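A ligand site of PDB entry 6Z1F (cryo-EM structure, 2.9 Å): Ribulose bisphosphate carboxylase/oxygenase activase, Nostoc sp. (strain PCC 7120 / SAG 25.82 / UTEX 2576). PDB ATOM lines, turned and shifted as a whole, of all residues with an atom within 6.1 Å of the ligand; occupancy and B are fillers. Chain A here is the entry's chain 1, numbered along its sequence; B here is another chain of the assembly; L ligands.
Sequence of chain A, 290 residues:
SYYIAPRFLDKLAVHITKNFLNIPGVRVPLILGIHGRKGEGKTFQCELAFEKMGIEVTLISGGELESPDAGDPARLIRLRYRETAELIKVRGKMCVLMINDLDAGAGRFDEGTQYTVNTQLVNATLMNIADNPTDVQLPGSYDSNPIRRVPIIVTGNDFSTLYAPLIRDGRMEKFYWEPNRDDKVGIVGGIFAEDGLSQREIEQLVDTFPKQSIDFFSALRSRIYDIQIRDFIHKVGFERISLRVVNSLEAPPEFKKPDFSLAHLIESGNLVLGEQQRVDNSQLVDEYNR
An oxygen (O2) of the ligand is in hydrogen-bond range of the backbone NH (N) of Lys 42 (3.4 Å).
An oxygen (O2) of the ligand lies within salt-bridge range of the side-chain amino group (NZ) of Lys 42.
N of Thr 43 sits at hydrogen-bond distance from O5 of the ligand (3.3 Å).
An oxygen (O1) of the ligand lies within hydrogen-bond range of the side-chain hydroxyl (OG1) of Thr 43 (2.9 Å).
O6 of the ligand sits at hydrogen-bond distance from N of Gly 41 (2.9 Å).
N of Phe 44 sits at hydrogen-bond distance from O5 of the ligand, at 2.9 Å.
The backbone NH (N) of Gly 39 is in hydrogen-bond range of an oxygen (O3) of the ligand (3.0 Å).
O2 of the ligand sits at hydrogen-bond distance from N of Glu 40, 3.1 Å away.
The backbone carbonyl oxygen (O) of Tyr 3 is in hydrogen-bond range of a nitrogen (N3) of the ligand (3.2 Å).
OD1 of Asp 215 sits at hydrogen-bond distance from O9 of the ligand (3.3 Å).
N3 of the ligand sits at hydrogen-bond distance from OE1 of Gln 45, 3.3 Å away.
The backbone carbonyl oxygen of Arg 37 sits at hydrogen-bond distance from the side-chain amino group of Lys 42, at 3.4 Å.
The backbone carbonyl oxygen (O) of Gly 39 lies within hydrogen-bond range of the backbone NH (N) of Asp 215 (3.0 Å).
O of Gly 39 lies within hydrogen-bond range of N of Ile 214, 3.0 Å away.
OE2 of Glu 40 lies within salt-bridge range of NE of Arg 37.
CD1 of Tyr 2 touches C9 of the ligand, at 3.6 Å.
Arg 37 touches the ligand (O to O2, 3.6 Å).
Lys 38 touches the ligand.
CG2 of Ile 187 touches C8 of the ligand (3.5 Å).
Ile 191 touches the ligand (CG1 to C9, 3.8 Å).
Ile 214 touches the ligand.
Ser 218 touches the ligand.
Within 4 Å of the ligand: Tyr 2, Tyr 3, Arg 37, Lys 38, Gly 39, Glu 40, Gly 41, Lys 42, Thr 43, Phe 44, Gln 45, Ile 187, Ile 191, Ile 214, Asp 215 and Ser 218.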
ATOM      1  N   TYR A   2      16.397 -19.414   2.043  1.00  0.00           N
ATOM      2  CA  TYR A   2      15.832 -19.696   3.347  1.00  0.00           C
ATOM      3  C   TYR A   2      16.921 -19.601   4.424  1.00  0.00           C
ATOM      4  O   TYR A   2      18.046 -20.021   4.213  1.00  0.00           O
ATOM      5  CB  TYR A   2      15.131 -21.065   3.353  1.00  0.00           C
ATOM      6  CG  TYR A   2      14.059 -21.197   2.310  1.00  0.00           C
ATOM      7  CD1 TYR A   2      12.832 -20.560   2.446  1.00  0.00           C
ATOM      8  CD2 TYR A   2      14.266 -21.968   1.175  1.00  0.00           C
ATOM      9  CE1 TYR A   2      11.837 -20.673   1.487  1.00  0.00           C
ATOM     10  CE2 TYR A   2      13.276 -22.098   0.199  1.00  0.00           C
ATOM     11  CZ  TYR A   2      12.069 -21.448   0.364  1.00  0.00           C
ATOM     12  OH  TYR A   2      11.091 -21.572  -0.586  1.00  0.00           O
ATOM     13  N   TYR A   3      16.522 -19.023   5.562  1.00  0.00           N
ATOM     14  CA  TYR A   3      17.407 -18.818   6.701  1.00  0.00           C
ATOM     15  C   TYR A   3      17.680 -20.152   7.384  1.00  0.00           C
ATOM     16  O   TYR A   3      16.791 -20.992   7.507  1.00  0.00           O
ATOM     17  CB  TYR A   3      16.769 -17.819   7.677  1.00  0.00           C
ATOM     18  CG  TYR A   3      17.582 -17.507   8.913  1.00  0.00           C
ATOM     19  CD1 TYR A   3      17.448 -18.268  10.063  1.00  0.00           C
ATOM     20  CD2 TYR A   3      18.455 -16.431   8.934  1.00  0.00           C
ATOM     21  CE1 TYR A   3      18.189 -17.976  11.206  1.00  0.00           C
ATOM     22  CE2 TYR A   3      19.191 -16.131  10.074  1.00  0.00           C
ATOM     23  CZ  TYR A   3      19.062 -16.909  11.207  1.00  0.00           C
ATOM     24  OH  TYR A   3      19.782 -16.614  12.329  1.00  0.00           O
ATOM     25  N   ILE A   4      18.930 -20.324   7.835  1.00  0.00           N
ATOM     26  CA  ILE A   4      19.302 -21.467   8.651  1.00  0.00           C
ATOM     27  C   ILE A   4      19.731 -20.940  10.023  1.00  0.00           C
ATOM     28  O   ILE A   4      20.494 -19.967  10.112  1.00  0.00           O
ATOM     29  CB  ILE A   4      20.404 -22.322   7.991  1.00  0.00           C
ATOM     30  CG1 ILE A   4      19.979 -22.858   6.623  1.00  0.00           C
ATOM     31  CG2 ILE A   4      20.856 -23.446   8.915  1.00  0.00           C
ATOM     32  CD1 ILE A   4      21.013 -23.736   5.949  1.00  0.00           C
ATOM     33  N   GLY A  36      12.332 -33.879  17.588  1.00  0.00           N
ATOM     34  CA  GLY A  36      11.567 -32.665  17.789  1.00  0.00           C
ATOM     35  C   GLY A  36      10.095 -32.856  17.397  1.00  0.00           C
ATOM     36  O   GLY A  36       9.715 -33.929  16.936  1.00  0.00           O
ATOM     37  N   ARG A  37       9.308 -31.804  17.602  1.00  0.00           N
ATOM     38  CA  ARG A  37       7.904 -31.772  17.195  1.00  0.00           C
ATOM     39  C   ARG A  37       7.816 -31.800  15.674  1.00  0.00           C
ATOM     40  O   ARG A  37       8.798 -31.520  14.983  1.00  0.00           O
ATOM     41  CB  ARG A  37       7.203 -30.540  17.770  1.00  0.00           C
ATOM     42  CG  ARG A  37       6.798 -30.671  19.228  1.00  0.00           C
ATOM     43  CD  ARG A  37       6.529 -29.307  19.834  1.00  0.00           C
ATOM     44  NE  ARG A  37       5.805 -28.440  18.911  1.00  0.00           N
ATOM     45  CZ  ARG A  37       5.722 -27.110  18.997  1.00  0.00           C
ATOM     46  NH1 ARG A  37       5.044 -26.431  18.088  1.00  0.00           N
ATOM     47  NH2 ARG A  37       6.320 -26.459  19.984  1.00  0.00           N
ATOM     48  N   LYS A  38       6.628 -32.150  15.161  1.00  0.00           N
ATOM     49  CA  LYS A  38       6.413 -32.284  13.723  1.00  0.00           C
ATOM     50  C   LYS A  38       6.250 -30.911  13.092  1.00  0.00           C
ATOM     51  O   LYS A  38       5.617 -30.026  13.660  1.00  0.00           O
ATOM     52  CB  LYS A  38       5.196 -33.177  13.454  1.00  0.00           C
ATOM     53  CG  LYS A  38       5.534 -34.634  13.186  1.00  0.00           C
ATOM     54  CD  LYS A  38       4.614 -35.619  13.886  1.00  0.00           C
ATOM     55  CE  LYS A  38       3.382 -35.994  13.075  1.00  0.00           C
ATOM     56  NZ  LYS A  38       2.678 -37.153  13.661  1.00  0.00           N
ATOM     57  N   GLY A  39       6.811 -30.767  11.884  1.00  0.00           N
ATOM     58  CA  GLY A  39       6.834 -29.502  11.160  1.00  0.00           C
ATOM     59  C   GLY A  39       7.708 -28.463  11.855  1.00  0.00           C
ATOM     60  O   GLY A  39       7.358 -27.292  11.898  1.00  0.00           O
ATOM     61  N   GLU A  40       8.828 -28.941  12.428  1.00  0.00           N
ATOM     62  CA  GLU A  40       9.833 -28.086  13.019  1.00  0.00           C
ATOM     63  C   GLU A  40      10.847 -27.663  11.959  1.00  0.00           C
ATOM     64  O   GLU A  40      11.482 -26.619  12.083  1.00  0.00           O
ATOM     65  CB  GLU A  40      10.552 -28.786  14.178  1.00  0.00           C
ATOM     66  CG  GLU A  40       9.847 -28.619  15.511  1.00  0.00           C
ATOM     67  CD  GLU A  40       9.338 -27.242  15.904  1.00  0.00           C
ATOM     68  OE1 GLU A  40       9.729 -26.241  15.254  1.00  0.00           O
ATOM     69  OE2 GLU A  40       8.551 -27.154  16.863  1.00  0.00           O
ATOM     70  N   GLY A  41      11.014 -28.519  10.951  1.00  0.00           N
ATOM     71  CA  GLY A  41      11.823 -28.191   9.787  1.00  0.00           C
ATOM     72  C   GLY A  41      13.200 -28.855   9.816  1.00  0.00           C
ATOM     73  O   GLY A  41      14.096 -28.415   9.099  1.00  0.00           O
ATOM     74  N   LYS A  42      13.322 -29.928  10.605  1.00  0.00           N
ATOM     75  CA  LYS A  42      14.568 -30.649  10.818  1.00  0.00           C
ATOM     76  C   LYS A  42      15.121 -31.204   9.500  1.00  0.00           C
ATOM     77  O   LYS A  42      16.317 -31.120   9.256  1.00  0.00           O
ATOM     78  CB  LYS A  42      14.345 -31.815  11.782  1.00  0.00           C
ATOM     79  CG  LYS A  42      14.074 -31.395  13.226  1.00  0.00           C
ATOM     80  CD  LYS A  42      14.059 -32.537  14.208  1.00  0.00           C
ATOM     81  CE  LYS A  42      12.976 -33.567  13.917  1.00  0.00           C
ATOM     82  NZ  LYS A  42      11.647 -32.959  13.708  1.00  0.00           N
ATOM     83  N   THR A  43      14.223 -31.768   8.693  1.00  0.00           N
ATOM     84  CA  THR A  43      14.539 -32.298   7.371  1.00  0.00           C
ATOM     85  C   THR A  43      14.925 -31.155   6.435  1.00  0.00           C
ATOM     86  O   THR A  43      15.839 -31.303   5.625  1.00  0.00           O
ATOM     87  CB  THR A  43      13.372 -33.118   6.806  1.00  0.00           C
ATOM     88  OG1 THR A  43      12.796 -33.898   7.850  1.00  0.00           O
ATOM     89  CG2 THR A  43      13.792 -34.018   5.670  1.00  0.00           C
ATOM     90  N   PHE A  44      14.213 -30.023   6.539  1.00  0.00           N
ATOM     91  CA  PHE A  44      14.409 -28.890   5.656  1.00  0.00           C
ATOM     92  C   PHE A  44      15.753 -28.218   5.924  1.00  0.00           C
ATOM     93  O   PHE A  44      16.413 -27.766   4.985  1.00  0.00           O
ATOM     94  CB  PHE A  44      13.273 -27.882   5.765  1.00  0.00           C
ATOM     95  CG  PHE A  44      13.112 -26.979   4.558  1.00  0.00           C
ATOM     96  CD1 PHE A  44      12.411 -27.421   3.443  1.00  0.00           C
ATOM     97  CD2 PHE A  44      13.662 -25.710   4.536  1.00  0.00           C
ATOM     98  CE1 PHE A  44      12.274 -26.604   2.324  1.00  0.00           C
ATOM     99  CE2 PHE A  44      13.521 -24.892   3.426  1.00  0.00           C
ATOM    100  CZ  PHE A  44      12.833 -25.337   2.317  1.00  0.00           C
ATOM    101  N   GLN A  45      16.136 -28.156   7.202  1.00  0.00           N
ATOM    102  CA  GLN A  45      17.385 -27.535   7.612  1.00  0.00           C
ATOM    103  C   GLN A  45      18.572 -28.381   7.151  1.00  0.00           C
ATOM    104  O   GLN A  45      19.575 -27.815   6.701  1.00  0.00           O
ATOM    105  CB  GLN A  45      17.449 -27.337   9.131  1.00  0.00           C
ATOM    106  CG  GLN A  45      16.322 -26.510   9.730  1.00  0.00           C
ATOM    107  CD  GLN A  45      16.455 -25.007   9.575  1.00  0.00           C
ATOM    108  OE1 GLN A  45      16.884 -24.501   8.543  1.00  0.00           O
ATOM    109  NE2 GLN A  45      16.067 -24.279  10.608  1.00  0.00           N
ATOM    110  N   LEU A  48      19.277 -27.963   3.402  1.00  0.00           N
ATOM    111  CA  LEU A  48      19.811 -26.642   3.136  1.00  0.00           C
ATOM    112  C   LEU A  48      21.289 -26.568   3.505  1.00  0.00           C
ATOM    113  O   LEU A  48      22.086 -26.055   2.723  1.00  0.00           O
ATOM    114  CB  LEU A  48      19.011 -25.614   3.941  1.00  0.00           C
ATOM    115  CG  LEU A  48      17.729 -25.101   3.306  1.00  0.00           C
ATOM    116  CD1 LEU A  48      17.080 -24.054   4.204  1.00  0.00           C
ATOM    117  CD2 LEU A  48      18.000 -24.512   1.922  1.00  0.00           C
ATOM    118  N   ASP A 101      12.231 -40.343   9.720  1.00  0.00           N
ATOM    119  CA  ASP A 101      11.122 -41.066  10.313  1.00  0.00           C
ATOM    120  C   ASP A 101      11.424 -42.561  10.375  1.00  0.00           C
ATOM    121  O   ASP A 101      10.760 -43.365   9.723  1.00  0.00           O
ATOM    122  CB  ASP A 101       9.804 -40.790   9.578  1.00  0.00           C
ATOM    123  CG  ASP A 101       9.289 -39.358   9.688  1.00  0.00           C
ATOM    124  OD1 ASP A 101       9.715 -38.647  10.627  1.00  0.00           O
ATOM    125  OD2 ASP A 101       8.465 -38.971   8.837  1.00  0.00           O
ATOM    126  N   THR A 155      16.584 -38.531  11.979  1.00  0.00           N
ATOM    127  CA  THR A 155      15.605 -37.594  12.503  1.00  0.00           C
ATOM    128  C   THR A 155      14.309 -38.324  12.844  1.00  0.00           C
ATOM    129  O   THR A 155      13.898 -39.233  12.127  1.00  0.00           O
ATOM    130  CB  THR A 155      15.315 -36.441  11.523  1.00  0.00           C
ATOM    131  OG1 THR A 155      14.807 -36.979  10.306  1.00  0.00           O
ATOM    132  CG2 THR A 155      16.517 -35.558  11.240  1.00  0.00           C
ATOM    133  N   ILE A 187      13.329 -17.684  10.110  1.00  0.00           N
ATOM    134  CA  ILE A 187      12.626 -18.602   9.239  1.00  0.00           C
ATOM    135  C   ILE A 187      11.405 -17.905   8.625  1.00  0.00           C
ATOM    136  O   ILE A 187      11.218 -17.958   7.405  1.00  0.00           O
ATOM    137  CB  ILE A 187      12.288 -19.927   9.960  1.00  0.00           C
ATOM    138  CG1 ILE A 187      13.565 -20.670  10.375  1.00  0.00           C
ATOM    139  CG2 ILE A 187      11.380 -20.803   9.106  1.00  0.00           C
ATOM    140  CD1 ILE A 187      13.404 -21.588  11.580  1.00  0.00           C
ATOM    141  N   ILE A 191      10.738 -16.790   4.461  1.00  0.00           N
ATOM    142  CA  ILE A 191       9.567 -17.244   3.730  1.00  0.00           C
ATOM    143  C   ILE A 191       8.905 -16.057   3.037  1.00  0.00           C
ATOM    144  O   ILE A 191       8.526 -16.149   1.863  1.00  0.00           O
ATOM    145  CB  ILE A 191       8.616 -18.013   4.670  1.00  0.00           C
ATOM    146  CG1 ILE A 191       9.179 -19.390   5.021  1.00  0.00           C
ATOM    147  CG2 ILE A 191       7.202 -18.111   4.114  1.00  0.00           C
ATOM    148  CD1 ILE A 191       8.655 -19.984   6.322  1.00  0.00           C
ATOM    149  N   ILE A 214       6.613 -24.560  12.978  1.00  0.00           N
ATOM    150  CA  ILE A 214       7.236 -23.837  11.875  1.00  0.00           C
ATOM    151  C   ILE A 214       6.406 -24.025  10.602  1.00  0.00           C
ATOM    152  O   ILE A 214       6.364 -23.123   9.762  1.00  0.00           O
ATOM    153  CB  ILE A 214       8.724 -24.255  11.695  1.00  0.00           C
ATOM    154  CG1 ILE A 214       9.581 -23.930  12.926  1.00  0.00           C
ATOM    155  CG2 ILE A 214       9.327 -23.705  10.412  1.00  0.00           C
ATOM    156  CD1 ILE A 214       9.642 -22.458  13.326  1.00  0.00           C
ATOM    157  N   ASP A 215       5.725 -25.173  10.508  1.00  0.00           N
ATOM    158  CA  ASP A 215       4.998 -25.586   9.322  1.00  0.00           C
ATOM    159  C   ASP A 215       3.770 -24.711   9.095  1.00  0.00           C
ATOM    160  O   ASP A 215       3.401 -24.464   7.941  1.00  0.00           O
ATOM    161  CB  ASP A 215       4.601 -27.063   9.395  1.00  0.00           C
ATOM    162  CG  ASP A 215       4.115 -27.655   8.074  1.00  0.00           C
ATOM    163  OD1 ASP A 215       4.580 -27.201   7.010  1.00  0.00           O
ATOM    164  OD2 ASP A 215       3.288 -28.584   8.127  1.00  0.00           O
ATOM    165  N   SER A 218       4.338 -21.319   7.160  1.00  0.00           N
ATOM    166  CA  SER A 218       4.604 -21.612   5.761  1.00  0.00           C
ATOM    167  C   SER A 218       3.296 -21.881   5.022  1.00  0.00           C
ATOM    168  O   SER A 218       3.157 -21.507   3.858  1.00  0.00           O
ATOM    169  CB  SER A 218       5.556 -22.765   5.640  1.00  0.00           C
ATOM    170  OG  SER A 218       5.740 -23.133   4.272  1.00  0.00           O
ATOM    171  N   ARG B 168      -2.804 -33.242   7.812  1.00  0.00           N
ATOM    172  CA  ARG B 168      -1.742 -32.252   7.761  1.00  0.00           C
ATOM    173  C   ARG B 168      -2.079 -31.187   6.730  1.00  0.00           C
ATOM    174  O   ARG B 168      -2.735 -31.479   5.732  1.00  0.00           O
ATOM    175  CB  ARG B 168      -0.397 -32.917   7.438  1.00  0.00           C
ATOM    176  CG  ARG B 168       0.257 -33.610   8.624  1.00  0.00           C
ATOM    177  CD  ARG B 168       1.583 -34.259   8.279  1.00  0.00           C
ATOM    178  NE  ARG B 168       2.642 -33.289   8.001  1.00  0.00           N
ATOM    179  CZ  ARG B 168       3.828 -33.575   7.478  1.00  0.00           C
ATOM    180  NH1 ARG B 168       4.709 -32.601   7.267  1.00  0.00           N
ATOM    181  NH2 ARG B 168       4.147 -34.815   7.160  1.00  0.00           N
HETATM  182  P1  LIG L   1      10.104 -32.068  10.545  1.00  0.00           P
HETATM  183  O1  LIG L   1      11.149 -33.005  10.015  1.00  0.00           O
HETATM  184  O2  LIG L   1      10.489 -31.441  11.861  1.00  0.00           O
HETATM  185  O3  LIG L   1       8.726 -32.679  10.571  1.00  0.00           O
HETATM  186  P2  LIG L   1      10.104 -30.849   7.882  1.00  0.00           P
HETATM  187  O4  LIG L   1       9.657 -32.177   7.386  1.00  0.00           O
HETATM  188  O5  LIG L   1      11.448 -30.357   7.464  1.00  0.00           O
HETATM  189  O6  LIG L   1      10.023 -30.854   9.490  1.00  0.00           O
HETATM  190  O7  LIG L   1       8.998 -29.745   7.540  1.00  0.00           O
HETATM  191  C1  LIG L   1       8.802 -29.344   6.162  1.00  0.00           C
HETATM  192  C2  LIG L   1       8.108 -28.002   6.112  1.00  0.00           C
HETATM  193  O8  LIG L   1       8.801 -27.068   6.976  1.00  0.00           O
HETATM  194  C3  LIG L   1       8.038 -27.323   4.735  1.00  0.00           C
HETATM  195  O9  LIG L   1       6.753 -26.753   4.518  1.00  0.00           O
HETATM  196  C4  LIG L   1       9.149 -26.270   4.795  1.00  0.00           C
HETATM  197  O10 LIG L   1       8.931 -25.143   3.979  1.00  0.00           O
HETATM  198  C5  LIG L   1       9.100 -25.886   6.271  1.00  0.00           C
HETATM  199  N1  LIG L   1      10.363 -25.335   6.763  1.00  0.00           N
HETATM  200  C6  LIG L   1      11.124 -25.858   7.772  1.00  0.00           C
HETATM  201  N2  LIG L   1      12.209 -25.178   8.029  1.00  0.00           N
HETATM  202  C7  LIG L   1      12.157 -24.118   7.129  1.00  0.00           C
HETATM  203  C8  LIG L   1      13.027 -23.036   6.897  1.00  0.00           C
HETATM  204  N3  LIG L   1      14.142 -22.833   7.586  1.00  0.00           N
HETATM  205  N4  LIG L   1      12.677 -22.152   5.931  1.00  0.00           N
HETATM  206  C9  LIG L   1      11.542 -22.365   5.246  1.00  0.00           C
HETATM  207  N5  LIG L   1      10.659 -23.350   5.370  1.00  0.00           N
HETATM  208  C10 LIG L   1      11.023 -24.207   6.349  1.00  0.00           C
